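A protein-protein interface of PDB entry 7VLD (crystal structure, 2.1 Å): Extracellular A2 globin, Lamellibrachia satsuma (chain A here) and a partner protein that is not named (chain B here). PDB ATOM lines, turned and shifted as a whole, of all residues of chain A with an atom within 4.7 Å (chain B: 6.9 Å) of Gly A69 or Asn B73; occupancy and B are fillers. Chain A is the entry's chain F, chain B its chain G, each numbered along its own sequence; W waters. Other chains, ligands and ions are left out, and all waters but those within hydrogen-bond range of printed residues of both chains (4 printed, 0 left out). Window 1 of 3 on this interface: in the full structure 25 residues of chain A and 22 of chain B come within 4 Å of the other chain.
Gly A69 touches just one residue of chain B: Asn B73. Printed residues of chain B within 4 Å of Arg A66: Gln B91. Of the printed residues of chain B, Thr A65 touches Ser B77. Of the printed residues of chain A, Trp B21 touches Asp A72 (3.5 Å). Of the printed residues of chain A, Ile B69 touches Met A73 (3.7 Å). The nearest residue of chain B that does not touch Gly A69 is Arg B29 (6.3 Å).
Water W3 lies within hydrogen-bond range of the side-chain amide oxygen (OD1) of Asn B73, the side-chain carboxylate (OD2) of Asp A72 and the guanidinium group (NH1) of Arg B29. Water W2 bridges the backbone carbonyl oxygen of Arg A66 (2.6 Å) and the side-chain amide nitrogen of Asn B73 (3.3 Å). Water W1 lies within hydrogen-bond range of the side-chain carboxylate (OD2) of Asp B76 (2.8 Å), the side-chain hydroxyl (OH) of Tyr A19 (2.9 Å) and the side-chain amide oxygen (OD1) of Asn B73 (3.3 Å). Water W4 lies within hydrogen-bond range of N of Ser B77 (3.3 Å), OD2 of Asp B76 (3.3 Å), O of Asn B73 (3.4 Å) and OH of Tyr A19 (3.5 Å).
Among the printed residues, merely in contact across the chains: Thr A65 with Ser B77, Asp A72 with Trp B21, Met A73 with Ile B69, Met A73 with Arg B70 and Met A73 with Asn B73.
Hydrophobic or aromatic side chains of chain B that line the printed part of chain A: Trp B21 and Ile B69. Of the 10 printed residues of chain A, 5 touch a printed residue of chain B. Hydrophobic or aromatic side chains of chain A within 4 Å of the printed part of chain B: Met A73. Among the printed residues, Asp or Glu carboxylates within 4 Å of a Lys or Arg side-chain nitrogen of the other chain: Asp A72 with Arg B29 (2.8 Å).
O of Gly B74 lies within hydrogen-bond range of OG of Ser B77 (2.6 Å). The side-chain hydroxyl (OG) of Ser B77 sits at hydrogen-bond distance from the side-chain amide nitrogen (NE2) of Gln B91 (3.2 Å).
NH1 of Arg B29 is in salt-bridge range of OD2 of Asp A72 (2.8 Å). O of Gly A69 sits close to OD1 of Asn B73 (3.2 Å). OE1 of Gln B91 sits at hydrogen-bond distance from NH2 of Arg A66, at 3.0 Å.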
ATOM      1  N   TYR A  19       2.988  10.509  -5.763  1.00  0.00           N
ATOM      2  CA  TYR A  19       3.925  11.513  -6.259  1.00  0.00           C
ATOM      3  C   TYR A  19       3.818  11.664  -7.772  1.00  0.00           C
ATOM      4  O   TYR A  19       3.918  12.779  -8.299  1.00  0.00           O
ATOM      5  CB  TYR A  19       5.345  11.127  -5.842  1.00  0.00           C
ATOM      6  CG  TYR A  19       6.392  12.207  -5.991  1.00  0.00           C
ATOM      7  CD1 TYR A  19       6.139  13.516  -5.601  1.00  0.00           C
ATOM      8  CD2 TYR A  19       7.652  11.903  -6.487  1.00  0.00           C
ATOM      9  CE1 TYR A  19       7.109  14.498  -5.727  1.00  0.00           C
ATOM     10  CE2 TYR A  19       8.624  12.872  -6.615  1.00  0.00           C
ATOM     11  CZ  TYR A  19       8.350  14.167  -6.234  1.00  0.00           C
ATOM     12  OH  TYR A  19       9.327  15.129  -6.365  1.00  0.00           O
ATOM     13  N   THR A  65       8.473  21.808  -3.549  1.00  0.00           N
ATOM     14  CA  THR A  65       9.121  20.917  -4.505  1.00  0.00           C
ATOM     15  C   THR A  65      10.371  20.289  -3.903  1.00  0.00           C
ATOM     16  O   THR A  65      10.621  19.090  -4.077  1.00  0.00           O
ATOM     17  CB  THR A  65       9.463  21.683  -5.784  1.00  0.00           C
ATOM     18  OG1 THR A  65       8.254  22.129  -6.414  1.00  0.00           O
ATOM     19  CG2 THR A  65      10.239  20.801  -6.753  1.00  0.00           C
ATOM     20  N   ARG A  66      11.162  21.082  -3.173  1.00  0.00           N
ATOM     21  CA  ARG A  66      12.378  20.556  -2.563  1.00  0.00           C
ATOM     22  C   ARG A  66      12.058  19.561  -1.454  1.00  0.00           C
ATOM     23  O   ARG A  66      12.732  18.533  -1.321  1.00  0.00           O
ATOM     24  CB  ARG A  66      13.237  21.704  -2.030  1.00  0.00           C
ATOM     25  CG  ARG A  66      13.735  22.651  -3.113  1.00  0.00           C
ATOM     26  CD  ARG A  66      14.784  23.626  -2.590  1.00  0.00           C
ATOM     27  NE  ARG A  66      14.212  24.684  -1.763  1.00  0.00           N
ATOM     28  CZ  ARG A  66      13.767  25.843  -2.238  1.00  0.00           C
ATOM     29  NH1 ARG A  66      13.266  26.752  -1.414  1.00  0.00           N
ATOM     30  NH2 ARG A  66      13.821  26.093  -3.540  1.00  0.00           N
ATOM     31  N   VAL A  67      11.028  19.845  -0.652  1.00  0.00           N
ATOM     32  CA  VAL A  67      10.645  18.933   0.423  1.00  0.00           C
ATOM     33  C   VAL A  67      10.218  17.587  -0.150  1.00  0.00           C
ATOM     34  O   VAL A  67      10.734  16.532   0.244  1.00  0.00           O
ATOM     35  CB  VAL A  67       9.533  19.555   1.288  1.00  0.00           C
ATOM     36  CG1 VAL A  67       9.079  18.569   2.352  1.00  0.00           C
ATOM     37  CG2 VAL A  67      10.019  20.844   1.923  1.00  0.00           C
ATOM     38  N   LEU A  68       9.273  17.602  -1.095  1.00  0.00           N
ATOM     39  CA  LEU A  68       8.804  16.352  -1.685  1.00  0.00           C
ATOM     40  C   LEU A  68       9.919  15.633  -2.433  1.00  0.00           C
ATOM     41  O   LEU A  68       9.946  14.398  -2.467  1.00  0.00           O
ATOM     42  CB  LEU A  68       7.620  16.611  -2.620  1.00  0.00           C
ATOM     43  CG  LEU A  68       6.375  17.285  -2.032  1.00  0.00           C
ATOM     44  CD1 LEU A  68       5.160  17.031  -2.915  1.00  0.00           C
ATOM     45  CD2 LEU A  68       6.113  16.828  -0.605  1.00  0.00           C
ATOM     46  N   GLY A  69      10.841  16.384  -3.040  1.00  0.00           N
ATOM     47  CA  GLY A  69      12.004  15.756  -3.645  1.00  0.00           C
ATOM     48  C   GLY A  69      12.872  15.049  -2.622  1.00  0.00           C
ATOM     49  O   GLY A  69      13.429  13.982  -2.895  1.00  0.00           O
ATOM     50  N   GLY A  70      12.993  15.631  -1.426  1.00  0.00           N
ATOM     51  CA  GLY A  70      13.727  14.964  -0.364  1.00  0.00           C
ATOM     52  C   GLY A  70      13.035  13.704   0.119  1.00  0.00           C
ATOM     53  O   GLY A  70      13.687  12.688   0.378  1.00  0.00           O
ATOM     54  N   LEU A  71      11.706  13.752   0.249  1.00  0.00           N
ATOM     55  CA  LEU A  71      10.955  12.548   0.590  1.00  0.00           C
ATOM     56  C   LEU A  71      11.118  11.478  -0.481  1.00  0.00           C
ATOM     57  O   LEU A  71      11.255  10.289  -0.167  1.00  0.00           O
ATOM     58  CB  LEU A  71       9.477  12.884   0.785  1.00  0.00           C
ATOM     59  CG  LEU A  71       9.060  13.393   2.163  1.00  0.00           C
ATOM     60  CD1 LEU A  71       7.616  13.853   2.135  1.00  0.00           C
ATOM     61  CD2 LEU A  71       9.254  12.302   3.200  1.00  0.00           C
ATOM     62  N   ASP A  72      11.109  11.884  -1.754  1.00  0.00           N
ATOM     63  CA  ASP A  72      11.249  10.921  -2.842  1.00  0.00           C
ATOM     64  C   ASP A  72      12.593  10.208  -2.781  1.00  0.00           C
ATOM     65  O   ASP A  72      12.669   8.993  -2.998  1.00  0.00           O
ATOM     66  CB  ASP A  72      11.081  11.623  -4.189  1.00  0.00           C
ATOM     67  CG  ASP A  72      11.155  10.661  -5.360  1.00  0.00           C
ATOM     68  OD1 ASP A  72      10.165   9.940  -5.600  1.00  0.00           O
ATOM     69  OD2 ASP A  72      12.204  10.622  -6.037  1.00  0.00           O
ATOM     70  N   MET A  73      13.667  10.947  -2.489  1.00  0.00           N
ATOM     71  CA  MET A  73      14.984  10.323  -2.394  1.00  0.00           C
ATOM     72  C   MET A  73      15.030   9.301  -1.265  1.00  0.00           C
ATOM     73  O   MET A  73      15.575   8.203  -1.434  1.00  0.00           O
ATOM     74  CB  MET A  73      16.060  11.391  -2.202  1.00  0.00           C
ATOM     75  CG  MET A  73      16.296  12.259  -3.429  1.00  0.00           C
ATOM     76  SD  MET A  73      17.653  13.432  -3.225  1.00  0.00           S
ATOM     77  CE  MET A  73      16.980  14.517  -1.971  1.00  0.00           C
ATOM     78  N   TRP B  17      12.508  12.160 -20.252  1.00  0.00           N
ATOM     79  CA  TRP B  17      12.890  11.939 -18.864  1.00  0.00           C
ATOM     80  C   TRP B  17      11.969  10.944 -18.167  1.00  0.00           C
ATOM     81  O   TRP B  17      12.431  10.173 -17.318  1.00  0.00           O
ATOM     82  CB  TRP B  17      12.897  13.273 -18.115  1.00  0.00           C
ATOM     83  CG  TRP B  17      13.490  13.219 -16.742  1.00  0.00           C
ATOM     84  CD1 TRP B  17      12.825  13.341 -15.558  1.00  0.00           C
ATOM     85  CD2 TRP B  17      14.872  13.036 -16.410  1.00  0.00           C
ATOM     86  NE1 TRP B  17      13.706  13.244 -14.508  1.00  0.00           N
ATOM     87  CE2 TRP B  17      14.969  13.057 -15.005  1.00  0.00           C
ATOM     88  CE3 TRP B  17      16.035  12.855 -17.163  1.00  0.00           C
ATOM     89  CZ2 TRP B  17      16.182  12.903 -14.338  1.00  0.00           C
ATOM     90  CZ3 TRP B  17      17.240  12.703 -16.500  1.00  0.00           C
ATOM     91  CH2 TRP B  17      17.303  12.728 -15.101  1.00  0.00           C
ATOM     92  N   TRP B  21      13.053   7.616 -16.068  1.00  0.00           N
ATOM     93  CA  TRP B  21      13.059   7.783 -14.620  1.00  0.00           C
ATOM     94  C   TRP B  21      12.280   6.662 -13.940  1.00  0.00           C
ATOM     95  O   TRP B  21      11.198   6.271 -14.390  1.00  0.00           O
ATOM     96  CB  TRP B  21      12.465   9.149 -14.269  1.00  0.00           C
ATOM     97  CG  TRP B  21      12.091   9.353 -12.832  1.00  0.00           C
ATOM     98  CD1 TRP B  21      10.951   8.928 -12.214  1.00  0.00           C
ATOM     99  CD2 TRP B  21      12.838  10.075 -11.845  1.00  0.00           C
ATOM    100  NE1 TRP B  21      10.951   9.321 -10.898  1.00  0.00           N
ATOM    101  CE2 TRP B  21      12.097  10.028 -10.646  1.00  0.00           C
ATOM    102  CE3 TRP B  21      14.063  10.748 -11.854  1.00  0.00           C
ATOM    103  CZ2 TRP B  21      12.541  10.629  -9.472  1.00  0.00           C
ATOM    104  CZ3 TRP B  21      14.503  11.343 -10.684  1.00  0.00           C
ATOM    105  CH2 TRP B  21      13.744  11.278  -9.511  1.00  0.00           C
ATOM    106  N   ARG B  29      18.184   5.558 -11.594  1.00  0.00           N
ATOM    107  CA  ARG B  29      18.664   6.915 -11.353  1.00  0.00           C
ATOM    108  C   ARG B  29      20.169   6.931 -11.136  1.00  0.00           C
ATOM    109  O   ARG B  29      20.879   7.776 -11.692  1.00  0.00           O
ATOM    110  CB  ARG B  29      17.969   7.523 -10.137  1.00  0.00           C
ATOM    111  CG  ARG B  29      16.468   7.340 -10.079  1.00  0.00           C
ATOM    112  CD  ARG B  29      15.941   7.975  -8.805  1.00  0.00           C
ATOM    113  NE  ARG B  29      14.510   7.773  -8.617  1.00  0.00           N
ATOM    114  CZ  ARG B  29      13.821   8.273  -7.597  1.00  0.00           C
ATOM    115  NH1 ARG B  29      14.437   9.009  -6.681  1.00  0.00           N
ATOM    116  NH2 ARG B  29      12.520   8.045  -7.495  1.00  0.00           N
ATOM    117  N   HIS B  67      25.177  11.821  -3.433  1.00  0.00           N
ATOM    118  CA  HIS B  67      25.303  13.035  -4.234  1.00  0.00           C
ATOM    119  C   HIS B  67      24.708  12.842  -5.624  1.00  0.00           C
ATOM    120  O   HIS B  67      24.027  13.735  -6.142  1.00  0.00           O
ATOM    121  CB  HIS B  67      26.768  13.455  -4.337  1.00  0.00           C
ATOM    122  CG  HIS B  67      27.005  14.560  -5.319  1.00  0.00           C
ATOM    123  ND1 HIS B  67      26.634  15.865  -5.075  1.00  0.00           N
ATOM    124  CD2 HIS B  67      27.558  14.550  -6.555  1.00  0.00           C
ATOM    125  CE1 HIS B  67      26.957  16.613  -6.114  1.00  0.00           C
ATOM    126  NE2 HIS B  67      27.519  15.840  -7.027  1.00  0.00           N
ATOM    127  N   CYS B  68      24.962  11.687  -6.245  1.00  0.00           N
ATOM    128  CA  CYS B  68      24.383  11.404  -7.555  1.00  0.00           C
ATOM    129  C   CYS B  68      22.861  11.447  -7.510  1.00  0.00           C
ATOM    130  O   CYS B  68      22.218  11.988  -8.418  1.00  0.00           O
ATOM    131  CB  CYS B  68      24.858  10.038  -8.055  1.00  0.00           C
ATOM    132  SG  CYS B  68      26.532  10.015  -8.727  1.00  0.00           S
ATOM    133  N   ILE B  69      22.270  10.882  -6.458  1.00  0.00           N
ATOM    134  CA  ILE B  69      20.817  10.865  -6.333  1.00  0.00           C
ATOM    135  C   ILE B  69      20.279  12.276  -6.127  1.00  0.00           C
ATOM    136  O   ILE B  69      19.217  12.632  -6.651  1.00  0.00           O
ATOM    137  CB  ILE B  69      20.407   9.910  -5.197  1.00  0.00           C
ATOM    138  CG1 ILE B  69      20.662   8.464  -5.629  1.00  0.00           C
ATOM    139  CG2 ILE B  69      18.953  10.117  -4.799  1.00  0.00           C
ATOM    140  CD1 ILE B  69      20.587   7.469  -4.509  1.00  0.00           C
ATOM    141  N   ARG B  70      21.009  13.108  -5.381  1.00  0.00           N
ATOM    142  CA  ARG B  70      20.588  14.495  -5.204  1.00  0.00           C
ATOM    143  C   ARG B  70      20.655  15.267  -6.516  1.00  0.00           C
ATOM    144  O   ARG B  70      19.791  16.107  -6.791  1.00  0.00           O
ATOM    145  CB  ARG B  70      21.444  15.178  -4.134  1.00  0.00           C
ATOM    146  CG  ARG B  70      21.194  14.672  -2.721  1.00  0.00           C
ATOM    147  CD  ARG B  70      21.842  15.566  -1.672  1.00  0.00           C
ATOM    148  NE  ARG B  70      23.302  15.483  -1.684  1.00  0.00           N
ATOM    149  CZ  ARG B  70      24.005  14.608  -0.972  1.00  0.00           C
ATOM    150  NH1 ARG B  70      23.385  13.732  -0.192  1.00  0.00           N
ATOM    151  NH2 ARG B  70      25.329  14.607  -1.042  1.00  0.00           N
ATOM    152  N   VAL B  71      21.672  14.995  -7.338  1.00  0.00           N
ATOM    153  CA  VAL B  71      21.816  15.708  -8.607  1.00  0.00           C
ATOM    154  C   VAL B  71      20.636  15.407  -9.523  1.00  0.00           C
ATOM    155  O   VAL B  71      19.979  16.318 -10.039  1.00  0.00           O
ATOM    156  CB  VAL B  71      23.155  15.355  -9.278  1.00  0.00           C
ATOM    157  CG1 VAL B  71      23.167  15.841 -10.719  1.00  0.00           C
ATOM    158  CG2 VAL B  71      24.314  15.962  -8.502  1.00  0.00           C
ATOM    159  N   VAL B  72      20.349  14.120  -9.741  1.00  0.00           N
ATOM    160  CA  VAL B  72      19.238  13.769 -10.619  1.00  0.00           C
ATOM    161  C   VAL B  72      17.910  14.194 -10.005  1.00  0.00           C
ATOM    162  O   VAL B  72      16.951  14.480 -10.732  1.00  0.00           O
ATOM    163  CB  VAL B  72      19.257  12.264 -10.950  1.00  0.00           C
ATOM    164  CG1 VAL B  72      20.459  11.933 -11.822  1.00  0.00           C
ATOM    165  CG2 VAL B  72      19.265  11.429  -9.681  1.00  0.00           C
ATOM    166  N   ASN B  73      17.826  14.254  -8.674  1.00  0.00           N
ATOM    167  CA  ASN B  73      16.635  14.818  -8.047  1.00  0.00           C
ATOM    168  C   ASN B  73      16.495  16.296  -8.385  1.00  0.00           C
ATOM    169  O   ASN B  73      15.388  16.779  -8.645  1.00  0.00           O
ATOM    170  CB  ASN B  73      16.682  14.617  -6.531  1.00  0.00           C
ATOM    171  CG  ASN B  73      15.489  15.237  -5.822  1.00  0.00           C
ATOM    172  OD1 ASN B  73      14.372  14.725  -5.900  1.00  0.00           O
ATOM    173  ND2 ASN B  73      15.724  16.341  -5.122  1.00  0.00           N
ATOM    174  N   GLY B  74      17.611  17.027  -8.395  1.00  0.00           N
ATOM    175  CA  GLY B  74      17.563  18.424  -8.791  1.00  0.00           C
ATOM    176  C   GLY B  74      17.175  18.604 -10.245  1.00  0.00           C
ATOM    177  O   GLY B  74      16.366  19.475 -10.578  1.00  0.00           O
ATOM    178  N   LEU B  75      17.744  17.786 -11.134  1.00  0.00           N
ATOM    179  CA  LEU B  75      17.375  17.871 -12.544  1.00  0.00           C
ATOM    180  C   LEU B  75      15.923  17.464 -12.755  1.00  0.00           C
ATOM    181  O   LEU B  75      15.213  18.073 -13.566  1.00  0.00           O
ATOM    182  CB  LEU B  75      18.308  17.002 -13.389  1.00  0.00           C
ATOM    183  CG  LEU B  75      18.038  17.005 -14.895  1.00  0.00           C
ATOM    184  CD1 LEU B  75      18.118  18.417 -15.459  1.00  0.00           C
ATOM    185  CD2 LEU B  75      19.005  16.078 -15.618  1.00  0.00           C
ATOM    186  N   ASP B  76      15.459  16.445 -12.025  1.00  0.00           N
ATOM    187  CA  ASP B  76      14.057  16.051 -12.111  1.00  0.00           C
ATOM    188  C   ASP B  76      13.138  17.181 -11.664  1.00  0.00           C
ATOM    189  O   ASP B  76      12.094  17.422 -12.281  1.00  0.00           O
ATOM    190  CB  ASP B  76      13.808  14.799 -11.269  1.00  0.00           C
ATOM    191  CG  ASP B  76      12.381  14.300 -11.374  1.00  0.00           C
ATOM    192  OD1 ASP B  76      12.026  13.742 -12.432  1.00  0.00           O
ATOM    193  OD2 ASP B  76      11.616  14.467 -10.400  1.00  0.00           O
ATOM    194  N   SER B  77      13.507  17.884 -10.590  1.00  0.00           N
ATOM    195  CA  SER B  77      12.690  19.001 -10.127  1.00  0.00           C
ATOM    196  C   SER B  77      12.635  20.106 -11.172  1.00  0.00           C
ATOM    197  O   SER B  77      11.591  20.739 -11.364  1.00  0.00           O
ATOM    198  CB  SER B  77      13.231  19.542  -8.803  1.00  0.00           C
ATOM    199  OG  SER B  77      14.421  20.288  -9.001  1.00  0.00           O
ATOM    200  N   ALA B  78      13.750  20.347 -11.865  1.00  0.00           N
ATOM    201  CA  ALA B  78      13.771  21.377 -12.897  1.00  0.00           C
ATOM    202  C   ALA B  78      12.959  20.950 -14.115  1.00  0.00           C
ATOM    203  O   ALA B  78      12.152  21.729 -14.638  1.00  0.00           O
ATOM    204  CB  ALA B  78      15.213  21.693 -13.290  1.00  0.00           C
ATOM    205  N   GLN B  91      13.177  27.876  -8.137  1.00  0.00           N
ATOM    206  CA  GLN B  91      13.964  26.679  -7.855  1.00  0.00           C
ATOM    207  C   GLN B  91      15.365  26.781  -8.443  1.00  0.00           C
ATOM    208  O   GLN B  91      16.337  26.326  -7.829  1.00  0.00           O
ATOM    209  CB  GLN B  91      13.243  25.441  -8.391  1.00  0.00           C
ATOM    210  CG  GLN B  91      14.031  24.139  -8.274  1.00  0.00           C
ATOM    211  CD  GLN B  91      14.141  23.632  -6.846  1.00  0.00           C
ATOM    212  OE1 GLN B  91      13.686  24.281  -5.903  1.00  0.00           O
ATOM    213  NE2 GLN B  91      14.744  22.461  -6.682  1.00  0.00           N
HETATM  214  O   HOH W   1      11.692  14.034  -7.613  1.00  0.00           O
HETATM  215  O   HOH W   2      15.067  18.234  -2.524  1.00  0.00           O
HETATM  216  O   HOH W   3      14.188  12.396  -6.614  1.00  0.00           O
HETATM  217  O   HOH W   4      12.099  16.591  -7.907  1.00  0.00           O
